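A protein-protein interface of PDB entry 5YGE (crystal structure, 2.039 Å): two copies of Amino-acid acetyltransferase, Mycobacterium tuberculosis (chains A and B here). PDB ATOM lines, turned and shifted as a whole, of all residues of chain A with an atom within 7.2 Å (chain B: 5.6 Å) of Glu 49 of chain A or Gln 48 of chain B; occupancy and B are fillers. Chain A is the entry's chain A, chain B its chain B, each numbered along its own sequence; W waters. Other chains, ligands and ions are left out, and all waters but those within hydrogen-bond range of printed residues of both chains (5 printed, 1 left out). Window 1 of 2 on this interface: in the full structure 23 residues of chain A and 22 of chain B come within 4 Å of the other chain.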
ATOM      1  N   ARG A  14     -31.200  -7.551 -10.395  1.00  0.00           N
ATOM      2  CA  ARG A  14     -29.837  -7.513 -10.798  1.00  0.00           C
ATOM      3  C   ARG A  14     -29.106  -8.788 -10.314  1.00  0.00           C
ATOM      4  O   ARG A  14     -29.312  -9.231  -9.235  1.00  0.00           O
ATOM      5  CB  ARG A  14     -29.146  -6.259 -10.303  1.00  0.00           C
ATOM      6  CG  ARG A  14     -29.595  -4.966 -10.953  1.00  0.00           C
ATOM      7  CD  ARG A  14     -28.770  -3.795 -10.511  1.00  0.00           C
ATOM      8  NE  ARG A  14     -29.273  -2.576 -11.080  1.00  0.00           N
ATOM      9  CZ  ARG A  14     -29.071  -2.179 -12.316  1.00  0.00           C
ATOM     10  NH1 ARG A  14     -28.366  -2.892 -13.136  1.00  0.00           N
ATOM     11  NH2 ARG A  14     -29.608  -1.066 -12.711  1.00  0.00           N
ATOM     12  N   ALA A  15     -28.310  -9.349 -11.182  1.00  0.00           N
ATOM     13  CA  ALA A  15     -27.423 -10.426 -10.843  1.00  0.00           C
ATOM     14  C   ALA A  15     -26.395 -10.082  -9.764  1.00  0.00           C
ATOM     15  O   ALA A  15     -25.992  -8.969  -9.611  1.00  0.00           O
ATOM     16  CB  ALA A  15     -26.743 -10.982 -12.056  1.00  0.00           C
ATOM     17  N   LEU A  43     -18.565 -14.604 -17.552  1.00  0.00           N
ATOM     18  CA  LEU A  43     -19.770 -14.351 -16.837  1.00  0.00           C
ATOM     19  C   LEU A  43     -19.525 -13.411 -15.628  1.00  0.00           C
ATOM     20  O   LEU A  43     -20.223 -12.484 -15.440  1.00  0.00           O
ATOM     21  CB  LEU A  43     -20.414 -15.658 -16.413  1.00  0.00           C
ATOM     22  CG  LEU A  43     -21.069 -16.515 -17.489  1.00  0.00           C
ATOM     23  CD1 LEU A  43     -21.668 -17.800 -16.960  1.00  0.00           C
ATOM     24  CD2 LEU A  43     -22.056 -15.746 -18.308  1.00  0.00           C
ATOM     25  N   GLU A  45     -17.121 -11.237 -15.151  1.00  0.00           N
ATOM     26  CA  GLU A  45     -16.802  -9.938 -15.645  1.00  0.00           C
ATOM     27  C   GLU A  45     -18.071  -9.191 -16.119  1.00  0.00           C
ATOM     28  O   GLU A  45     -18.207  -8.048 -15.890  1.00  0.00           O
ATOM     29  CB  GLU A  45     -15.777  -9.993 -16.758  1.00  0.00           C
ATOM     30  CG  GLU A  45     -14.385 -10.402 -16.364  1.00  0.00           C
ATOM     31  CD  GLU A  45     -13.508 -10.646 -17.580  1.00  0.00           C
ATOM     32  OE1 GLU A  45     -13.882 -10.219 -18.674  1.00  0.00           O
ATOM     33  OE2 GLU A  45     -12.490 -11.270 -17.451  1.00  0.00           O
ATOM     34  N   ALA A  46     -18.989  -9.916 -16.725  1.00  0.00           N
ATOM     35  CA  ALA A  46     -20.195  -9.356 -17.276  1.00  0.00           C
ATOM     36  C   ALA A  46     -21.367  -9.301 -16.315  1.00  0.00           C
ATOM     37  O   ALA A  46     -22.439  -8.979 -16.707  1.00  0.00           O
ATOM     38  CB  ALA A  46     -20.596 -10.128 -18.512  1.00  0.00           C
ATOM     39  N   VAL A  47     -21.142  -9.642 -15.061  1.00  0.00           N
ATOM     40  CA  VAL A  47     -22.190  -9.818 -14.101  1.00  0.00           C
ATOM     41  C   VAL A  47     -23.128  -8.599 -13.977  1.00  0.00           C
ATOM     42  O   VAL A  47     -24.302  -8.741 -13.858  1.00  0.00           O
ATOM     43  CB  VAL A  47     -21.671 -10.277 -12.733  1.00  0.00           C
ATOM     44  CG1 VAL A  47     -20.911  -9.188 -12.010  1.00  0.00           C
ATOM     45  CG2 VAL A  47     -22.788 -10.888 -11.937  1.00  0.00           C
ATOM     46  N   GLN A  48     -22.555  -7.441 -14.061  1.00  0.00           N
ATOM     47  CA  GLN A  48     -23.292  -6.236 -13.932  1.00  0.00           C
ATOM     48  C   GLN A  48     -24.220  -5.941 -15.119  1.00  0.00           C
ATOM     49  O   GLN A  48     -25.008  -5.100 -15.030  1.00  0.00           O
ATOM     50  CB  GLN A  48     -22.367  -5.073 -13.571  1.00  0.00           C
ATOM     51  CG  GLN A  48     -21.555  -5.288 -12.314  1.00  0.00           C
ATOM     52  CD  GLN A  48     -20.792  -4.071 -11.883  1.00  0.00           C
ATOM     53  OE1 GLN A  48     -21.323  -3.217 -11.269  1.00  0.00           O
ATOM     54  NE2 GLN A  48     -19.549  -4.034 -12.214  1.00  0.00           N
ATOM     55  N   GLU A  49     -24.131  -6.674 -16.196  1.00  0.00           N
ATOM     56  CA  GLU A  49     -25.034  -6.594 -17.323  1.00  0.00           C
ATOM     57  C   GLU A  49     -26.276  -7.521 -17.195  1.00  0.00           C
ATOM     58  O   GLU A  49     -27.197  -7.423 -17.937  1.00  0.00           O
ATOM     59  CB  GLU A  49     -24.265  -6.958 -18.609  1.00  0.00           C
ATOM     60  CG  GLU A  49     -23.256  -5.961 -19.042  1.00  0.00           C
ATOM     61  CD  GLU A  49     -22.537  -6.314 -20.317  1.00  0.00           C
ATOM     62  OE1 GLU A  49     -22.778  -7.299 -20.964  1.00  0.00           O
ATOM     63  OE2 GLU A  49     -21.691  -5.572 -20.664  1.00  0.00           O
ATOM     64  N   PHE A  50     -26.188  -8.451 -16.264  1.00  0.00           N
ATOM     65  CA  PHE A  50     -27.118  -9.533 -16.092  1.00  0.00           C
ATOM     66  C   PHE A  50     -28.266  -9.257 -15.135  1.00  0.00           C
ATOM     67  O   PHE A  50     -28.085  -8.665 -14.129  1.00  0.00           O
ATOM     68  CB  PHE A  50     -26.400 -10.790 -15.656  1.00  0.00           C
ATOM     69  CG  PHE A  50     -25.939 -11.636 -16.780  1.00  0.00           C
ATOM     70  CD1 PHE A  50     -24.713 -11.448 -17.328  1.00  0.00           C
ATOM     71  CD2 PHE A  50     -26.767 -12.560 -17.345  1.00  0.00           C
ATOM     72  CE1 PHE A  50     -24.292 -12.221 -18.379  1.00  0.00           C
ATOM     73  CE2 PHE A  50     -26.363 -13.338 -18.395  1.00  0.00           C
ATOM     74  CZ  PHE A  50     -25.119 -13.181 -18.904  1.00  0.00           C
ATOM     75  N   TRP A  51     -29.436  -9.722 -15.512  1.00  0.00           N
ATOM     76  CA  TRP A  51     -30.598  -9.738 -14.679  1.00  0.00           C
ATOM     77  C   TRP A  51     -31.073 -11.203 -14.505  1.00  0.00           C
ATOM     78  O   TRP A  51     -30.877 -12.000 -15.370  1.00  0.00           O
ATOM     79  CB  TRP A  51     -31.716  -8.814 -15.184  1.00  0.00           C
ATOM     80  CG  TRP A  51     -31.345  -7.372 -15.202  1.00  0.00           C
ATOM     81  CD1 TRP A  51     -30.497  -6.817 -16.026  1.00  0.00           C
ATOM     82  CD2 TRP A  51     -31.806  -6.333 -14.350  1.00  0.00           C
ATOM     83  NE1 TRP A  51     -30.353  -5.522 -15.769  1.00  0.00           N
ATOM     84  CE2 TRP A  51     -31.151  -5.179 -14.736  1.00  0.00           C
ATOM     85  CE3 TRP A  51     -32.664  -6.271 -13.272  1.00  0.00           C
ATOM     86  CZ2 TRP A  51     -31.345  -3.968 -14.109  1.00  0.00           C
ATOM     87  CZ3 TRP A  51     -32.872  -5.058 -12.666  1.00  0.00           C
ATOM     88  CH2 TRP A  51     -32.207  -3.934 -13.079  1.00  0.00           C
ATOM     89  N   GLY A  66     -30.977 -12.985 -18.251  1.00  0.00           N
ATOM     90  CA  GLY A  66     -30.750 -12.250 -19.450  1.00  0.00           C
ATOM     91  C   GLY A  66     -29.795 -11.105 -19.257  1.00  0.00           C
ATOM     92  O   GLY A  66     -29.638 -10.653 -18.208  1.00  0.00           O
ATOM     93  N   ALA A  67     -29.192 -10.653 -20.317  1.00  0.00           N
ATOM     94  CA  ALA A  67     -28.274  -9.545 -20.298  1.00  0.00           C
ATOM     95  C   ALA A  67     -28.436  -8.521 -21.435  1.00  0.00           C
ATOM     96  O   ALA A  67     -28.863  -8.819 -22.497  1.00  0.00           O
ATOM     97  CB  ALA A  67     -26.858 -10.046 -20.252  1.00  0.00           C
ATOM     98  N   LEU A  68     -27.997  -7.320 -21.164  1.00  0.00           N
ATOM     99  CA  LEU A  68     -27.893  -6.292 -22.120  1.00  0.00           C
ATOM    100  C   LEU A  68     -26.462  -5.713 -22.143  1.00  0.00           C
ATOM    101  O   LEU A  68     -25.888  -5.383 -21.138  1.00  0.00           O
ATOM    102  CB  LEU A  68     -28.876  -5.198 -21.821  1.00  0.00           C
ATOM    103  CG  LEU A  68     -28.863  -3.950 -22.696  1.00  0.00           C
ATOM    104  CD1 LEU A  68     -29.553  -4.181 -24.014  1.00  0.00           C
ATOM    105  CD2 LEU A  68     -29.494  -2.794 -21.993  1.00  0.00           C
ATOM    106  N   HIS A  69     -25.949  -5.626 -23.334  1.00  0.00           N
ATOM    107  CA  HIS A  69     -24.628  -5.166 -23.573  1.00  0.00           C
ATOM    108  C   HIS A  69     -24.656  -3.914 -24.413  1.00  0.00           C
ATOM    109  O   HIS A  69     -25.312  -3.897 -25.389  1.00  0.00           O
ATOM    110  CB  HIS A  69     -23.823  -6.243 -24.252  1.00  0.00           C
ATOM    111  CG  HIS A  69     -22.446  -5.819 -24.575  1.00  0.00           C
ATOM    112  ND1 HIS A  69     -21.461  -5.736 -23.631  1.00  0.00           N
ATOM    113  CD2 HIS A  69     -21.893  -5.408 -25.730  1.00  0.00           C
ATOM    114  CE1 HIS A  69     -20.356  -5.318 -24.204  1.00  0.00           C
ATOM    115  NE2 HIS A  69     -20.604  -5.082 -25.465  1.00  0.00           N
ATOM    116  N   VAL A  70     -23.967  -2.882 -23.964  1.00  0.00           N
ATOM    117  CA  VAL A  70     -23.957  -1.598 -24.660  1.00  0.00           C
ATOM    118  C   VAL A  70     -22.775  -1.611 -25.634  1.00  0.00           C
ATOM    119  O   VAL A  70     -21.649  -1.925 -25.240  1.00  0.00           O
ATOM    120  CB  VAL A  70     -23.817  -0.443 -23.645  1.00  0.00           C
ATOM    121  CG1 VAL A  70     -23.551   0.905 -24.340  1.00  0.00           C
ATOM    122  CG2 VAL A  70     -25.059  -0.348 -22.780  1.00  0.00           C
ATOM    123  N   GLU A  77     -27.245  -4.567 -27.374  1.00  0.00           N
ATOM    124  CA  GLU A  77     -27.563  -5.923 -27.790  1.00  0.00           C
ATOM    125  C   GLU A  77     -28.054  -6.784 -26.627  1.00  0.00           C
ATOM    126  O   GLU A  77     -27.479  -6.793 -25.573  1.00  0.00           O
ATOM    127  CB  GLU A  77     -26.384  -6.608 -28.441  1.00  0.00           C
ATOM    128  CG  GLU A  77     -26.630  -8.038 -28.865  1.00  0.00           C
ATOM    129  CD  GLU A  77     -25.418  -8.795 -29.437  1.00  0.00           C
ATOM    130  OE1 GLU A  77     -24.281  -8.376 -29.258  1.00  0.00           O
ATOM    131  OE2 GLU A  77     -25.595  -9.816 -30.059  1.00  0.00           O
ATOM    132  N   ARG A  79     -28.461 -10.301 -24.991  1.00  0.00           N
ATOM    133  CA  ARG A  79     -27.716 -11.530 -24.945  1.00  0.00           C
ATOM    134  C   ARG A  79     -28.138 -12.499 -23.840  1.00  0.00           C
ATOM    135  O   ARG A  79     -28.614 -12.095 -22.828  1.00  0.00           O
ATOM    136  CB  ARG A  79     -26.237 -11.268 -24.767  1.00  0.00           C
ATOM    137  CG  ARG A  79     -25.617 -10.211 -25.642  1.00  0.00           C
ATOM    138  CD  ARG A  79     -24.135 -10.149 -25.428  1.00  0.00           C
ATOM    139  NE  ARG A  79     -23.464  -9.339 -26.397  1.00  0.00           N
ATOM    140  CZ  ARG A  79     -22.225  -8.887 -26.284  1.00  0.00           C
ATOM    141  NH1 ARG A  79     -21.490  -9.175 -25.239  1.00  0.00           N
ATOM    142  NH2 ARG A  79     -21.723  -8.173 -27.249  1.00  0.00           N
ATOM    143  N   LEU A 100     -34.895  -5.825 -19.509  1.00  0.00           N
ATOM    144  CA  LEU A 100     -33.755  -5.424 -20.330  1.00  0.00           C
ATOM    145  C   LEU A 100     -34.084  -4.201 -21.190  1.00  0.00           C
ATOM    146  O   LEU A 100     -33.329  -3.300 -21.304  1.00  0.00           O
ATOM    147  CB  LEU A 100     -33.265  -6.551 -21.195  1.00  0.00           C
ATOM    148  CG  LEU A 100     -32.914  -7.831 -20.490  1.00  0.00           C
ATOM    149  CD1 LEU A 100     -32.455  -8.962 -21.374  1.00  0.00           C
ATOM    150  CD2 LEU A 100     -31.899  -7.519 -19.439  1.00  0.00           C
ATOM    151  N   VAL A 103     -34.212  -1.199 -19.172  1.00  0.00           N
ATOM    152  CA  VAL A 103     -32.865  -0.809 -18.851  1.00  0.00           C
ATOM    153  C   VAL A 103     -32.293  -0.011 -20.024  1.00  0.00           C
ATOM    154  O   VAL A 103     -31.648   0.941 -19.832  1.00  0.00           O
ATOM    155  CB  VAL A 103     -31.966  -2.008 -18.521  1.00  0.00           C
ATOM    156  CG1 VAL A 103     -30.519  -1.573 -18.433  1.00  0.00           C
ATOM    157  CG2 VAL A 103     -32.370  -2.629 -17.205  1.00  0.00           C
ATOM    158  N   LEU A 107     -30.900   3.748 -19.880  1.00  0.00           N
ATOM    159  CA  LEU A 107     -29.539   4.027 -20.325  1.00  0.00           C
ATOM    160  C   LEU A 107     -29.395   5.056 -21.456  1.00  0.00           C
ATOM    161  O   LEU A 107     -28.327   5.532 -21.726  1.00  0.00           O
ATOM    162  CB  LEU A 107     -28.829   2.729 -20.695  1.00  0.00           C
ATOM    163  CG  LEU A 107     -28.333   1.775 -19.634  1.00  0.00           C
ATOM    164  CD1 LEU A 107     -27.863   0.508 -20.261  1.00  0.00           C
ATOM    165  CD2 LEU A 107     -27.273   2.357 -18.754  1.00  0.00           C
ATOM    166  N   ARG B  14     -26.184   5.567 -11.082  1.00  0.00           N
ATOM    167  CA  ARG B  14     -25.675   4.848 -12.207  1.00  0.00           C
ATOM    168  C   ARG B  14     -25.618   5.714 -13.449  1.00  0.00           C
ATOM    169  O   ARG B  14     -26.503   6.435 -13.732  1.00  0.00           O
ATOM    170  CB  ARG B  14     -26.505   3.610 -12.492  1.00  0.00           C
ATOM    171  CG  ARG B  14     -26.498   2.530 -11.436  1.00  0.00           C
ATOM    172  CD  ARG B  14     -27.192   1.305 -11.927  1.00  0.00           C
ATOM    173  NE  ARG B  14     -27.270   0.271 -10.936  1.00  0.00           N
ATOM    174  CZ  ARG B  14     -26.280  -0.542 -10.627  1.00  0.00           C
ATOM    175  NH1 ARG B  14     -25.141  -0.451 -11.211  1.00  0.00           N
ATOM    176  NH2 ARG B  14     -26.436  -1.406  -9.687  1.00  0.00           N
ATOM    177  N   TYR B  44     -18.372   3.413 -23.314  1.00  0.00           N
ATOM    178  CA  TYR B  44     -19.701   2.974 -23.646  1.00  0.00           C
ATOM    179  C   TYR B  44     -19.934   1.518 -23.218  1.00  0.00           C
ATOM    180  O   TYR B  44     -20.852   1.231 -22.566  1.00  0.00           O
ATOM    181  CB  TYR B  44     -20.066   3.218 -25.105  1.00  0.00           C
ATOM    182  CG  TYR B  44     -20.345   4.680 -25.432  1.00  0.00           C
ATOM    183  CD1 TYR B  44     -21.291   5.380 -24.727  1.00  0.00           C
ATOM    184  CD2 TYR B  44     -19.638   5.355 -26.392  1.00  0.00           C
ATOM    185  CE1 TYR B  44     -21.547   6.668 -24.983  1.00  0.00           C
ATOM    186  CE2 TYR B  44     -19.893   6.662 -26.659  1.00  0.00           C
ATOM    187  CZ  TYR B  44     -20.847   7.323 -25.932  1.00  0.00           C
ATOM    188  OH  TYR B  44     -21.117   8.608 -26.098  1.00  0.00           O
ATOM    189  N   GLU B  45     -19.028   0.643 -23.595  1.00  0.00           N
ATOM    190  CA  GLU B  45     -19.099  -0.754 -23.242  1.00  0.00           C
ATOM    191  C   GLU B  45     -19.077  -1.025 -21.744  1.00  0.00           C
ATOM    192  O   GLU B  45     -19.657  -1.906 -21.305  1.00  0.00           O
ATOM    193  CB  GLU B  45     -17.985  -1.544 -23.862  1.00  0.00           C
ATOM    194  CG  GLU B  45     -18.093  -1.737 -25.343  1.00  0.00           C
ATOM    195  CD  GLU B  45     -16.973  -2.616 -25.850  1.00  0.00           C
ATOM    196  OE1 GLU B  45     -16.754  -3.651 -25.262  1.00  0.00           O
ATOM    197  OE2 GLU B  45     -16.306  -2.248 -26.790  1.00  0.00           O
ATOM    198  N   ALA B  46     -18.423  -0.174 -21.005  1.00  0.00           N
ATOM    199  CA  ALA B  46     -18.280  -0.274 -19.578  1.00  0.00           C
ATOM    200  C   ALA B  46     -19.303   0.532 -18.774  1.00  0.00           C
ATOM    201  O   ALA B  46     -19.236   0.563 -17.584  1.00  0.00           O
ATOM    202  CB  ALA B  46     -16.871   0.130 -19.200  1.00  0.00           C
ATOM    203  N   VAL B  47     -20.223   1.173 -19.464  1.00  0.00           N
ATOM    204  CA  VAL B  47     -21.115   2.105 -18.871  1.00  0.00           C
ATOM    205  C   VAL B  47     -21.849   1.587 -17.618  1.00  0.00           C
ATOM    206  O   VAL B  47     -21.983   2.276 -16.689  1.00  0.00           O
ATOM    207  CB  VAL B  47     -22.067   2.742 -19.887  1.00  0.00           C
ATOM    208  CG1 VAL B  47     -23.179   1.801 -20.292  1.00  0.00           C
ATOM    209  CG2 VAL B  47     -22.525   4.082 -19.399  1.00  0.00           C
ATOM    210  N   GLN B  48     -22.203   0.330 -17.660  1.00  0.00           N
ATOM    211  CA  GLN B  48     -22.917  -0.364 -16.597  1.00  0.00           C
ATOM    212  C   GLN B  48     -22.086  -0.646 -15.324  1.00  0.00           C
ATOM    213  O   GLN B  48     -22.595  -1.072 -14.370  1.00  0.00           O
ATOM    214  CB  GLN B  48     -23.642  -1.601 -17.137  1.00  0.00           C
ATOM    215  CG  GLN B  48     -24.590  -1.287 -18.269  1.00  0.00           C
ATOM    216  CD  GLN B  48     -25.440  -2.446 -18.650  1.00  0.00           C
ATOM    217  OE1 GLN B  48     -26.328  -2.768 -17.952  1.00  0.00           O
ATOM    218  NE2 GLN B  48     -25.112  -3.090 -19.719  1.00  0.00           N
ATOM    219  N   GLU B  49     -20.803  -0.381 -15.405  1.00  0.00           N
ATOM    220  CA  GLU B  49     -19.873  -0.428 -14.313  1.00  0.00           C
ATOM    221  C   GLU B  49     -19.724   0.922 -13.586  1.00  0.00           C
ATOM    222  O   GLU B  49     -19.188   0.968 -12.524  1.00  0.00           O
ATOM    223  CB  GLU B  49     -18.484  -0.863 -14.796  1.00  0.00           C
ATOM    224  CG  GLU B  49     -18.442  -2.221 -15.414  1.00  0.00           C
ATOM    225  CD  GLU B  49     -17.056  -2.753 -15.670  1.00  0.00           C
ATOM    226  OE1 GLU B  49     -16.120  -2.000 -15.708  1.00  0.00           O
ATOM    227  OE2 GLU B  49     -16.926  -3.929 -15.850  1.00  0.00           O
ATOM    228  N   PHE B  50     -20.138   1.972 -14.277  1.00  0.00           N
ATOM    229  CA  PHE B  50     -19.956   3.358 -13.909  1.00  0.00           C
ATOM    230  C   PHE B  50     -21.101   4.014 -13.137  1.00  0.00           C
ATOM    231  O   PHE B  50     -22.254   3.840 -13.418  1.00  0.00           O
ATOM    232  CB  PHE B  50     -19.670   4.233 -15.116  1.00  0.00           C
ATOM    233  CG  PHE B  50     -18.245   4.325 -15.496  1.00  0.00           C
ATOM    234  CD1 PHE B  50     -17.437   5.261 -14.941  1.00  0.00           C
ATOM    235  CD2 PHE B  50     -17.705   3.452 -16.394  1.00  0.00           C
ATOM    236  CE1 PHE B  50     -16.128   5.365 -15.299  1.00  0.00           C
ATOM    237  CE2 PHE B  50     -16.386   3.537 -16.744  1.00  0.00           C
ATOM    238  CZ  PHE B  50     -15.605   4.508 -16.205  1.00  0.00           C
ATOM    239  N   TRP B  51     -20.681   4.783 -12.170  1.00  0.00           N
ATOM    240  CA  TRP B  51     -21.508   5.635 -11.402  1.00  0.00           C
ATOM    241  C   TRP B  51     -20.964   7.063 -11.534  1.00  0.00           C
ATOM    242  O   TRP B  51     -19.793   7.265 -11.714  1.00  0.00           O
ATOM    243  CB  TRP B  51     -21.586   5.179  -9.959  1.00  0.00           C
ATOM    244  CG  TRP B  51     -22.215   3.795  -9.717  1.00  0.00           C
ATOM    245  CD1 TRP B  51     -21.726   2.618 -10.067  1.00  0.00           C
ATOM    246  CD2 TRP B  51     -23.431   3.534  -9.052  1.00  0.00           C
ATOM    247  NE1 TRP B  51     -22.546   1.626  -9.699  1.00  0.00           N
ATOM    248  CE2 TRP B  51     -23.615   2.156  -9.063  1.00  0.00           C
ATOM    249  CE3 TRP B  51     -24.405   4.331  -8.484  1.00  0.00           C
ATOM    250  CZ2 TRP B  51     -24.714   1.563  -8.515  1.00  0.00           C
ATOM    251  CZ3 TRP B  51     -25.475   3.737  -7.933  1.00  0.00           C
ATOM    252  CH2 TRP B  51     -25.624   2.373  -7.947  1.00  0.00           C
HETATM  253  O   HOH W   1     -28.354  -4.787 -17.804  1.00  0.00           O
HETATM  254  O   HOH W   2     -21.317  -0.592 -10.852  1.00  0.00           O
HETATM  255  O   HOH W   3     -17.629  -5.722 -14.078  1.00  0.00           O
HETATM  256  O   HOH W   4     -24.030  -3.267 -10.345  1.00  0.00           O
HETATM  257  O   HOH W   5     -22.550  -3.051 -21.366  1.00  0.00           O
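Of the 20 printed residues of chain A, 5 touch a printed residue of chain B.
Printed residues of chain A that touch a printed residue of chain B: Arg 14, Gln 48, Glu 49, Leu 68 and Val 70.
Hydrophobic or aromatic side chains of chain A within 4 Å of the printed part of chain B: Val 70.
Among the printed residues, no Asp or Glu carboxylate lies within 4 Å of a Lys or Arg side-chain nitrogen of the other chain.
The backbone carbonyl oxygen of Glu 49 of chain A lies within hydrogen-bond range of the backbone NH of Leu 68 of chain A.
The side-chain carboxylate (OE2) of Glu 49 of chain A lies within hydrogen-bond range of a ring nitrogen (ND1) of His 69 of chain A (3.0 Å).
Water W3 lies within hydrogen-bond range of OE2 of Glu 49 of chain B (2.6 Å), O of Glu 45 of chain A (3.0 Å) and NE2 of Gln 48 of chain A (3.2 Å).
Water W2 lies within hydrogen-bond range of the side-chain amide oxygen of Gln 48 of chain A (2.7 Å), the indole nitrogen of Trp 51 of chain B (2.8 Å) and the backbone carbonyl oxygen of Glu 49 of chain B (3.1 Å).
Water W5 lies within hydrogen-bond range of the side-chain carboxylate of Glu 49 of chain A (2.8 Å), the backbone NH of Val 70 of chain A (3.0 Å), the side-chain amide nitrogen of Gln 48 of chain B (3.0 Å) and the backbone carbonyl oxygen of Glu 45 of chain B (3.1 Å).
Water W4 bridges the side-chain amide oxygen (OE1) of Gln 48 of chain A (2.9 Å) and the guanidinium group (NH2) of Arg 14 of chain B (3.1 Å).
Water W1 lies within hydrogen-bond range of the side-chain amide oxygen of Gln 48 of chain B, the backbone carbonyl oxygen of Glu 49 of chain A and the indole nitrogen of Trp 51 of chain A.
Gln 48 of chain A touches Gln 48 of chain B (O to OE1, 3.96 Å).
Gln 48 of chain A touches Glu 49 of chain B (NE2 to CG, 3.8 Å).
NE2 of Gln 48 of chain B touches CG of Glu 49 of chain A (3.5 Å).
Val 70 of chain A touches Tyr 44 of chain B.
O of Val 70 of chain A touches CA of Glu 45 of chain B, 3.4 Å away.
CG2 of Val 70 of chain A touches CG1 of Val 47 of chain B, at 3.8 Å.
Of the printed residues of chain B, Arg 14 of chain A touches Arg 14.
Of chain B, only Gln 48 comes within 4 Å of Glu 49 of chain A.
Of the printed residues of chain A, Val 47 of chain B touches Val 70.
Gln 48 of chain B touches just these residues of chain A: Gln 48, Glu 49 and Leu 68.
The nearest residue of chain B that does not touch Glu 49 of chain A is Glu 45 of chain B (4.2 Å).
The nearest residue of chain A that does not touch Gln 48 of chain B is Val 70 of chain A (4.1 Å).
The nearest printed residue of chain A that does not touch Glu 45 of chain B is His 69 of chain A (4.1 Å).
The guanidinium group (NH2) of Arg 14 of chain A lies close to the guanidinium group (NE) of Arg 14 of chain B, 3.2 Å away.
The backbone carbonyl oxygen (O) of Leu 68 of chain A lies within hydrogen-bond range of the side-chain amide nitrogen (NE2) of Gln 48 of chain B (2.8 Å).
Arg 14 of chain B touches its own counterpart, Arg 14 of chain A.
Gln 48 of chain B touches its own counterpart, Gln 48 of chain A.
Gln 48 of chain A touches Glu 49 of chain B, and with the chains exchanged Glu 49 of chain A touches Gln 48 of chain B.
Of the 8 pairs that touch across the chains among the printed residues, 4 have their exchanged pair printed and touching as well.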
